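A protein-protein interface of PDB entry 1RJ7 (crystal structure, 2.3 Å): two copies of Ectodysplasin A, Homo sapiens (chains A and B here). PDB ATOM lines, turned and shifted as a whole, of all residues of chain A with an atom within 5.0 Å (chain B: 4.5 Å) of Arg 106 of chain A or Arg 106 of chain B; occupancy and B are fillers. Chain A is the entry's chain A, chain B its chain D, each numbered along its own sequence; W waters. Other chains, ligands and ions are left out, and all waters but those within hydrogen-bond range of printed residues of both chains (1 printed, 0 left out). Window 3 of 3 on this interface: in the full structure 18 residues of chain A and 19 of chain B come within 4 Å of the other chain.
NH1 of Arg 106 of chain A lies close to NH1 of Arg 106 of chain B (3.0 Å). The backbone NH of Thr 117 of chain B lies within hydrogen-bond range of the backbone carbonyl oxygen of Thr 105 of chain A, at 2.9 Å. The backbone NH (N) of Ser 107 of chain A lies within hydrogen-bond range of the side-chain amide oxygen (OD1) of Asn 116 of chain B, at 3.0 Å. The backbone carbonyl oxygen of Tyr 115 of chain B is in hydrogen-bond range of the side-chain hydroxyl of Ser 107 of chain A (2.9 Å).
Water W1 lies within hydrogen-bond range of the side-chain hydroxyl (OG1) of Thr 117 of chain B (2.9 Å) and the side-chain sulfur (SG) of Cys 104 of chain A (3.7 Å).
Of the 12 printed residues of chain A, 5 touch a printed residue of chain B. Along chain A the printed residues that touch a printed residue of chain B span positions 89 to 107. Among the printed residues, no Asp or Glu carboxylate lies within 4 Å of a Lys or Arg side-chain nitrogen of the other chain.
Printed residues of chain B within 4 Å of Phe 89 of chain A: Tyr 115 (3.99 Å). Printed residues of chain B within 4 Å of Cys 104 of chain A: Thr 117. Printed residues of chain B within 4 Å of Thr 105 of chain A: Tyr 115, Asn 116 and Thr 117. Of chain B, only Arg 106 (3.0 Å), Tyr 115 (3.7 Å) and Asn 116 (3.4 Å) come within 4 Å of Arg 106 of chain A. Of the printed residues of chain A, Arg 106 of chain B touches Arg 106 (3.0 Å). Of the printed residues of chain A, Asn 116 of chain B touches Thr 105, Arg 106 and Ser 107.
Thr 105 of chain A touches Asn 116 of chain B, but with the chains exchanged Asn 116 of chain A does not touch Thr 105 of chain B (10.6 Å). Thr 105 of chain A touches Thr 117 of chain B, but with the chains exchanged Thr 117 of chain A does not touch Thr 105 of chain B (10.7 Å). Arg 106 of chain A touches Asn 116 of chain B, but with the chains exchanged Asn 116 of chain A does not touch Arg 106 of chain B (6.2 Å). Ser 107 of chain A touches Asn 116 of chain B, but with the chains exchanged Asn 116 of chain A does not touch Ser 107 of chain B (8.4 Å).
Among the printed residues, merely in contact across the chains: Arg 106 of chain A with Asn 116 of chain B (3.4 Å), Thr 105 of chain A with Asn 116 of chain B (3.4 Å), Thr 105 of chain A with Tyr 115 of chain B (3.5 Å), Cys 104 of chain A with Thr 117 of chain B (3.6 Å), Arg 106 of chain A with Tyr 115 of chain B (3.7 Å) and Phe 89 of chain A with Tyr 115 of chain B (3.99 Å).
The guanidinium group (NH1) of Arg 106 of chain A is in hydrogen-bond range of the side-chain amide oxygen (OD1) of Asn 116 of chain A. The side-chain sulfur (SG) of Cys 118 of chain B lies within hydrogen-bond range of the backbone carbonyl oxygen (O) of Asn 116 of chain B (3.5 Å). The backbone carbonyl oxygen (O) of Arg 106 of chain A sits at hydrogen-bond distance from the backbone NH (N) of Ala 90 of chain A (2.8 Å). O of Asp 88 of chain A lies close to OG of Ser 107 of chain A. NH1 of Arg 106 of chain B lies within hydrogen-bond range of OD1 of Asn 116 of chain B (3.1 Å). NH2 of Arg 106 of chain B lies within hydrogen-bond range of O of Thr 117 of chain B.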
ATOM      1  N   ILE A  84     -21.173 -34.725 -17.375  1.00  0.00           N
ATOM      2  CA  ILE A  84     -20.777 -35.803 -18.254  1.00  0.00           C
ATOM      3  C   ILE A  84     -20.964 -37.082 -17.473  1.00  0.00           C
ATOM      4  O   ILE A  84     -20.486 -37.233 -16.345  1.00  0.00           O
ATOM      5  CB  ILE A  84     -19.332 -35.650 -18.774  1.00  0.00           C
ATOM      6  CG1 ILE A  84     -19.190 -34.363 -19.578  1.00  0.00           C
ATOM      7  CG2 ILE A  84     -18.983 -36.814 -19.678  1.00  0.00           C
ATOM      8  CD1 ILE A  84     -17.755 -34.039 -19.976  1.00  0.00           C
ATOM      9  N   ASP A  88     -15.274 -38.396 -19.186  1.00  0.00           N
ATOM     10  CA  ASP A  88     -14.224 -37.395 -18.932  1.00  0.00           C
ATOM     11  C   ASP A  88     -13.804 -36.614 -20.189  1.00  0.00           C
ATOM     12  O   ASP A  88     -12.661 -36.168 -20.304  1.00  0.00           O
ATOM     13  CB  ASP A  88     -13.029 -37.985 -18.119  1.00  0.00           C
ATOM     14  CG  ASP A  88     -11.997 -38.764 -18.964  1.00  0.00           C
ATOM     15  OD1 ASP A  88     -12.035 -38.768 -20.217  1.00  0.00           O
ATOM     16  OD2 ASP A  88     -11.069 -39.405 -18.415  1.00  0.00           O
ATOM     17  N   PHE A  89     -14.755 -36.414 -21.100  1.00  0.00           N
ATOM     18  CA  PHE A  89     -14.468 -35.870 -22.425  1.00  0.00           C
ATOM     19  C   PHE A  89     -15.754 -35.393 -23.123  1.00  0.00           C
ATOM     20  O   PHE A  89     -16.573 -36.191 -23.580  1.00  0.00           O
ATOM     21  CB  PHE A  89     -13.756 -36.947 -23.256  1.00  0.00           C
ATOM     22  CG  PHE A  89     -13.582 -36.614 -24.720  1.00  0.00           C
ATOM     23  CD1 PHE A  89     -12.443 -35.958 -25.169  1.00  0.00           C
ATOM     24  CD2 PHE A  89     -14.526 -37.019 -25.663  1.00  0.00           C
ATOM     25  CE1 PHE A  89     -12.264 -35.680 -26.526  1.00  0.00           C
ATOM     26  CE2 PHE A  89     -14.351 -36.744 -27.016  1.00  0.00           C
ATOM     27  CZ  PHE A  89     -13.221 -36.075 -27.449  1.00  0.00           C
ATOM     28  N   ALA A  90     -15.940 -34.087 -23.172  1.00  0.00           N
ATOM     29  CA  ALA A  90     -17.005 -33.490 -23.967  1.00  0.00           C
ATOM     30  C   ALA A  90     -16.359 -32.938 -25.225  1.00  0.00           C
ATOM     31  O   ALA A  90     -15.296 -32.338 -25.169  1.00  0.00           O
ATOM     32  CB  ALA A  90     -17.713 -32.375 -23.201  1.00  0.00           C
ATOM     33  N   CYS A 104     -13.757 -28.674 -30.693  1.00  0.00           N
ATOM     34  CA  CYS A 104     -13.530 -28.182 -29.345  1.00  0.00           C
ATOM     35  C   CYS A 104     -13.615 -29.368 -28.422  1.00  0.00           C
ATOM     36  O   CYS A 104     -14.589 -30.106 -28.462  1.00  0.00           O
ATOM     37  CB  CYS A 104     -14.636 -27.179 -28.988  1.00  0.00           C
ATOM     38  SG  CYS A 104     -14.391 -26.319 -27.411  1.00  0.00           S
ATOM     39  N   THR A 105     -12.604 -29.568 -27.592  1.00  0.00           N
ATOM     40  CA  THR A 105     -12.640 -30.653 -26.635  1.00  0.00           C
ATOM     41  C   THR A 105     -12.317 -30.190 -25.233  1.00  0.00           C
ATOM     42  O   THR A 105     -11.420 -29.402 -25.015  1.00  0.00           O
ATOM     43  CB  THR A 105     -11.647 -31.735 -27.029  1.00  0.00           C
ATOM     44  OG1 THR A 105     -10.309 -31.238 -26.895  1.00  0.00           O
ATOM     45  CG2 THR A 105     -11.780 -32.105 -28.502  1.00  0.00           C
ATOM     46  N   ARG A 106     -13.023 -30.739 -24.266  1.00  0.00           N
ATOM     47  CA  ARG A 106     -12.739 -30.439 -22.880  1.00  0.00           C
ATOM     48  C   ARG A 106     -12.857 -31.707 -22.075  1.00  0.00           C
ATOM     49  O   ARG A 106     -13.750 -32.511 -22.308  1.00  0.00           O
ATOM     50  CB  ARG A 106     -13.727 -29.393 -22.347  1.00  0.00           C
ATOM     51  CG  ARG A 106     -13.403 -28.913 -20.943  1.00  0.00           C
ATOM     52  CD  ARG A 106     -14.323 -27.846 -20.457  1.00  0.00           C
ATOM     53  NE  ARG A 106     -14.082 -26.584 -21.167  1.00  0.00           N
ATOM     54  CZ  ARG A 106     -13.409 -25.568 -20.665  1.00  0.00           C
ATOM     55  NH1 ARG A 106     -12.911 -25.654 -19.450  1.00  0.00           N
ATOM     56  NH2 ARG A 106     -13.210 -24.465 -21.378  1.00  0.00           N
ATOM     57  N   SER A 107     -11.965 -31.870 -21.117  1.00  0.00           N
ATOM     58  CA  SER A 107     -12.014 -33.000 -20.210  1.00  0.00           C
ATOM     59  C   SER A 107     -12.590 -32.551 -18.869  1.00  0.00           C
ATOM     60  O   SER A 107     -12.023 -31.676 -18.205  1.00  0.00           O
ATOM     61  CB  SER A 107     -10.616 -33.580 -20.027  1.00  0.00           C
ATOM     62  OG  SER A 107     -10.119 -34.033 -21.277  1.00  0.00           O
ATOM     63  N   ILE A 108     -13.723 -33.153 -18.497  1.00  0.00           N
ATOM     64  CA  ILE A 108     -14.465 -32.789 -17.286  1.00  0.00           C
ATOM     65  C   ILE A 108     -14.726 -34.037 -16.464  1.00  0.00           C
ATOM     66  O   ILE A 108     -15.183 -35.045 -17.002  1.00  0.00           O
ATOM     67  CB  ILE A 108     -15.810 -32.127 -17.661  1.00  0.00           C
ATOM     68  CG1 ILE A 108     -15.580 -30.843 -18.438  1.00  0.00           C
ATOM     69  CG2 ILE A 108     -16.650 -31.834 -16.433  1.00  0.00           C
ATOM     70  CD1 ILE A 108     -16.821 -30.381 -19.192  1.00  0.00           C
ATOM     71  N   ASN A 116     -18.977 -25.841 -17.543  1.00  0.00           N
ATOM     72  CA  ASN A 116     -17.861 -25.326 -18.341  1.00  0.00           C
ATOM     73  C   ASN A 116     -18.327 -24.847 -19.702  1.00  0.00           C
ATOM     74  O   ASN A 116     -18.898 -25.635 -20.478  1.00  0.00           O
ATOM     75  CB  ASN A 116     -16.806 -26.414 -18.555  1.00  0.00           C
ATOM     76  CG  ASN A 116     -16.085 -26.773 -17.287  1.00  0.00           C
ATOM     77  OD1 ASN A 116     -15.191 -26.053 -16.856  1.00  0.00           O
ATOM     78  ND2 ASN A 116     -16.467 -27.884 -16.679  1.00  0.00           N
ATOM     79  N   THR A 117     -18.106 -23.573 -20.004  1.00  0.00           N
ATOM     80  CA  THR A 117     -18.325 -23.101 -21.378  1.00  0.00           C
ATOM     81  C   THR A 117     -17.156 -23.481 -22.275  1.00  0.00           C
ATOM     82  O   THR A 117     -16.002 -23.348 -21.909  1.00  0.00           O
ATOM     83  CB  THR A 117     -18.579 -21.589 -21.480  1.00  0.00           C
ATOM     84  OG1 THR A 117     -17.558 -20.865 -20.775  1.00  0.00           O
ATOM     85  CG2 THR A 117     -19.919 -21.214 -20.849  1.00  0.00           C
ATOM     86  N   CYS A 118     -17.508 -23.918 -23.479  1.00  0.00           N
ATOM     87  CA  CYS A 118     -16.576 -24.506 -24.428  1.00  0.00           C
ATOM     88  C   CYS A 118     -16.596 -23.716 -25.738  1.00  0.00           C
ATOM     89  O   CYS A 118     -17.484 -23.913 -26.593  1.00  0.00           O
ATOM     90  CB  CYS A 118     -16.962 -25.972 -24.661  1.00  0.00           C
ATOM     91  SG  CYS A 118     -16.947 -26.961 -23.159  1.00  0.00           S
ATOM     92  N   ASP B  88       1.312 -29.403 -13.434  1.00  0.00           N
ATOM     93  CA  ASP B  88      -0.119 -29.531 -13.745  1.00  0.00           C
ATOM     94  C   ASP B  88      -0.655 -28.365 -14.587  1.00  0.00           C
ATOM     95  O   ASP B  88      -1.855 -28.283 -14.855  1.00  0.00           O
ATOM     96  CB  ASP B  88      -0.947 -29.738 -12.461  1.00  0.00           C
ATOM     97  CG  ASP B  88      -0.624 -28.731 -11.369  1.00  0.00           C
ATOM     98  OD1 ASP B  88       0.005 -27.696 -11.661  1.00  0.00           O
ATOM     99  OD2 ASP B  88      -0.968 -28.887 -10.182  1.00  0.00           O
ATOM    100  N   PHE B  89       0.265 -27.515 -15.050  1.00  0.00           N
ATOM    101  CA  PHE B  89      -0.033 -26.246 -15.700  1.00  0.00           C
ATOM    102  C   PHE B  89       0.438 -26.314 -17.148  1.00  0.00           C
ATOM    103  O   PHE B  89       1.639 -26.280 -17.420  1.00  0.00           O
ATOM    104  CB  PHE B  89       0.669 -25.117 -14.923  1.00  0.00           C
ATOM    105  CG  PHE B  89       0.651 -23.775 -15.605  1.00  0.00           C
ATOM    106  CD1 PHE B  89      -0.518 -23.028 -15.667  1.00  0.00           C
ATOM    107  CD2 PHE B  89       1.823 -23.234 -16.139  1.00  0.00           C
ATOM    108  CE1 PHE B  89      -0.525 -21.780 -16.276  1.00  0.00           C
ATOM    109  CE2 PHE B  89       1.819 -21.981 -16.752  1.00  0.00           C
ATOM    110  CZ  PHE B  89       0.640 -21.254 -16.820  1.00  0.00           C
ATOM    111  N   ALA B  90      -0.521 -26.463 -18.059  1.00  0.00           N
ATOM    112  CA  ALA B  90      -0.293 -26.288 -19.484  1.00  0.00           C
ATOM    113  C   ALA B  90      -0.515 -24.832 -19.856  1.00  0.00           C
ATOM    114  O   ALA B  90      -1.417 -24.178 -19.345  1.00  0.00           O
ATOM    115  CB  ALA B  90      -1.222 -27.166 -20.288  1.00  0.00           C
ATOM    116  N   THR B 105      -3.789 -20.309 -20.509  1.00  0.00           N
ATOM    117  CA  THR B 105      -3.438 -21.254 -19.460  1.00  0.00           C
ATOM    118  C   THR B 105      -4.622 -22.173 -19.139  1.00  0.00           C
ATOM    119  O   THR B 105      -5.787 -21.774 -19.241  1.00  0.00           O
ATOM    120  CB  THR B 105      -2.992 -20.506 -18.167  1.00  0.00           C
ATOM    121  OG1 THR B 105      -4.117 -19.910 -17.509  1.00  0.00           O
ATOM    122  CG2 THR B 105      -2.046 -19.326 -18.478  1.00  0.00           C
ATOM    123  N   ARG B 106      -4.310 -23.403 -18.741  1.00  0.00           N
ATOM    124  CA  ARG B 106      -5.320 -24.378 -18.376  1.00  0.00           C
ATOM    125  C   ARG B 106      -4.786 -25.455 -17.435  1.00  0.00           C
ATOM    126  O   ARG B 106      -3.631 -25.880 -17.565  1.00  0.00           O
ATOM    127  CB  ARG B 106      -5.878 -25.052 -19.622  1.00  0.00           C
ATOM    128  CG  ARG B 106      -7.059 -25.940 -19.297  1.00  0.00           C
ATOM    129  CD  ARG B 106      -7.575 -26.660 -20.451  1.00  0.00           C
ATOM    130  NE  ARG B 106      -8.292 -25.738 -21.317  1.00  0.00           N
ATOM    131  CZ  ARG B 106      -9.599 -25.704 -21.442  1.00  0.00           C
ATOM    132  NH1 ARG B 106     -10.362 -26.546 -20.746  1.00  0.00           N
ATOM    133  NH2 ARG B 106     -10.147 -24.820 -22.263  1.00  0.00           N
ATOM    134  N   SER B 107      -5.657 -25.918 -16.529  1.00  0.00           N
ATOM    135  CA  SER B 107      -5.353 -26.992 -15.572  1.00  0.00           C
ATOM    136  C   SER B 107      -5.907 -28.322 -16.082  1.00  0.00           C
ATOM    137  O   SER B 107      -7.087 -28.407 -16.448  1.00  0.00           O
ATOM    138  CB  SER B 107      -5.993 -26.700 -14.214  1.00  0.00           C
ATOM    139  OG  SER B 107      -5.440 -25.539 -13.621  1.00  0.00           O
ATOM    140  N   ILE B 108      -5.045 -29.337 -16.128  1.00  0.00           N
ATOM    141  CA  ILE B 108      -5.403 -30.687 -16.594  1.00  0.00           C
ATOM    142  C   ILE B 108      -4.699 -31.709 -15.720  1.00  0.00           C
ATOM    143  O   ILE B 108      -3.534 -31.527 -15.373  1.00  0.00           O
ATOM    144  CB  ILE B 108      -4.937 -30.890 -18.065  1.00  0.00           C
ATOM    145  CG1 ILE B 108      -5.757 -30.041 -19.031  1.00  0.00           C
ATOM    146  CG2 ILE B 108      -5.038 -32.356 -18.480  1.00  0.00           C
ATOM    147  CD1 ILE B 108      -4.985 -29.641 -20.286  1.00  0.00           C
ATOM    148  N   TYR B 115      -7.798 -34.802 -23.213  1.00  0.00           N
ATOM    149  CA  TYR B 115      -7.827 -33.916 -24.379  1.00  0.00           C
ATOM    150  C   TYR B 115      -8.509 -32.583 -24.048  1.00  0.00           C
ATOM    151  O   TYR B 115      -9.689 -32.564 -23.689  1.00  0.00           O
ATOM    152  CB  TYR B 115      -8.547 -34.592 -25.553  1.00  0.00           C
ATOM    153  CG  TYR B 115      -7.762 -35.719 -26.171  1.00  0.00           C
ATOM    154  CD1 TYR B 115      -6.777 -35.465 -27.121  1.00  0.00           C
ATOM    155  CD2 TYR B 115      -7.988 -37.040 -25.792  1.00  0.00           C
ATOM    156  CE1 TYR B 115      -6.035 -36.503 -27.688  1.00  0.00           C
ATOM    157  CE2 TYR B 115      -7.252 -38.087 -26.350  1.00  0.00           C
ATOM    158  CZ  TYR B 115      -6.274 -37.806 -27.299  1.00  0.00           C
ATOM    159  OH  TYR B 115      -5.536 -38.818 -27.869  1.00  0.00           O
ATOM    160  N   ASN B 116      -7.764 -31.483 -24.174  1.00  0.00           N
ATOM    161  CA  ASN B 116      -8.284 -30.138 -23.912  1.00  0.00           C
ATOM    162  C   ASN B 116      -7.792 -29.107 -24.939  1.00  0.00           C
ATOM    163  O   ASN B 116      -6.592 -28.873 -25.068  1.00  0.00           O
ATOM    164  CB  ASN B 116      -7.904 -29.684 -22.488  1.00  0.00           C
ATOM    165  CG  ASN B 116      -8.859 -30.212 -21.421  1.00  0.00           C
ATOM    166  OD1 ASN B 116      -9.925 -29.632 -21.173  1.00  0.00           O
ATOM    167  ND2 ASN B 116      -8.471 -31.301 -20.765  1.00  0.00           N
ATOM    168  N   THR B 117      -8.721 -28.491 -25.663  1.00  0.00           N
ATOM    169  CA  THR B 117      -8.387 -27.392 -26.567  1.00  0.00           C
ATOM    170  C   THR B 117      -8.400 -26.061 -25.824  1.00  0.00           C
ATOM    171  O   THR B 117      -9.337 -25.738 -25.115  1.00  0.00           O
ATOM    172  CB  THR B 117      -9.336 -27.312 -27.764  1.00  0.00           C
ATOM    173  OG1 THR B 117     -10.696 -27.306 -27.322  1.00  0.00           O
ATOM    174  CG2 THR B 117      -9.187 -28.531 -28.653  1.00  0.00           C
ATOM    175  N   CYS B 118      -7.339 -25.290 -26.039  1.00  0.00           N
ATOM    176  CA  CYS B 118      -7.028 -24.112 -25.255  1.00  0.00           C
ATOM    177  C   CYS B 118      -6.933 -22.969 -26.243  1.00  0.00           C
ATOM    178  O   CYS B 118      -5.944 -22.858 -26.973  1.00  0.00           O
ATOM    179  CB  CYS B 118      -5.715 -24.330 -24.516  1.00  0.00           C
ATOM    180  SG  CYS B 118      -5.663 -25.847 -23.517  1.00  0.00           S
HETATM  181  O   HOH W   1     -11.151 -24.512 -27.663  1.00  0.00           O
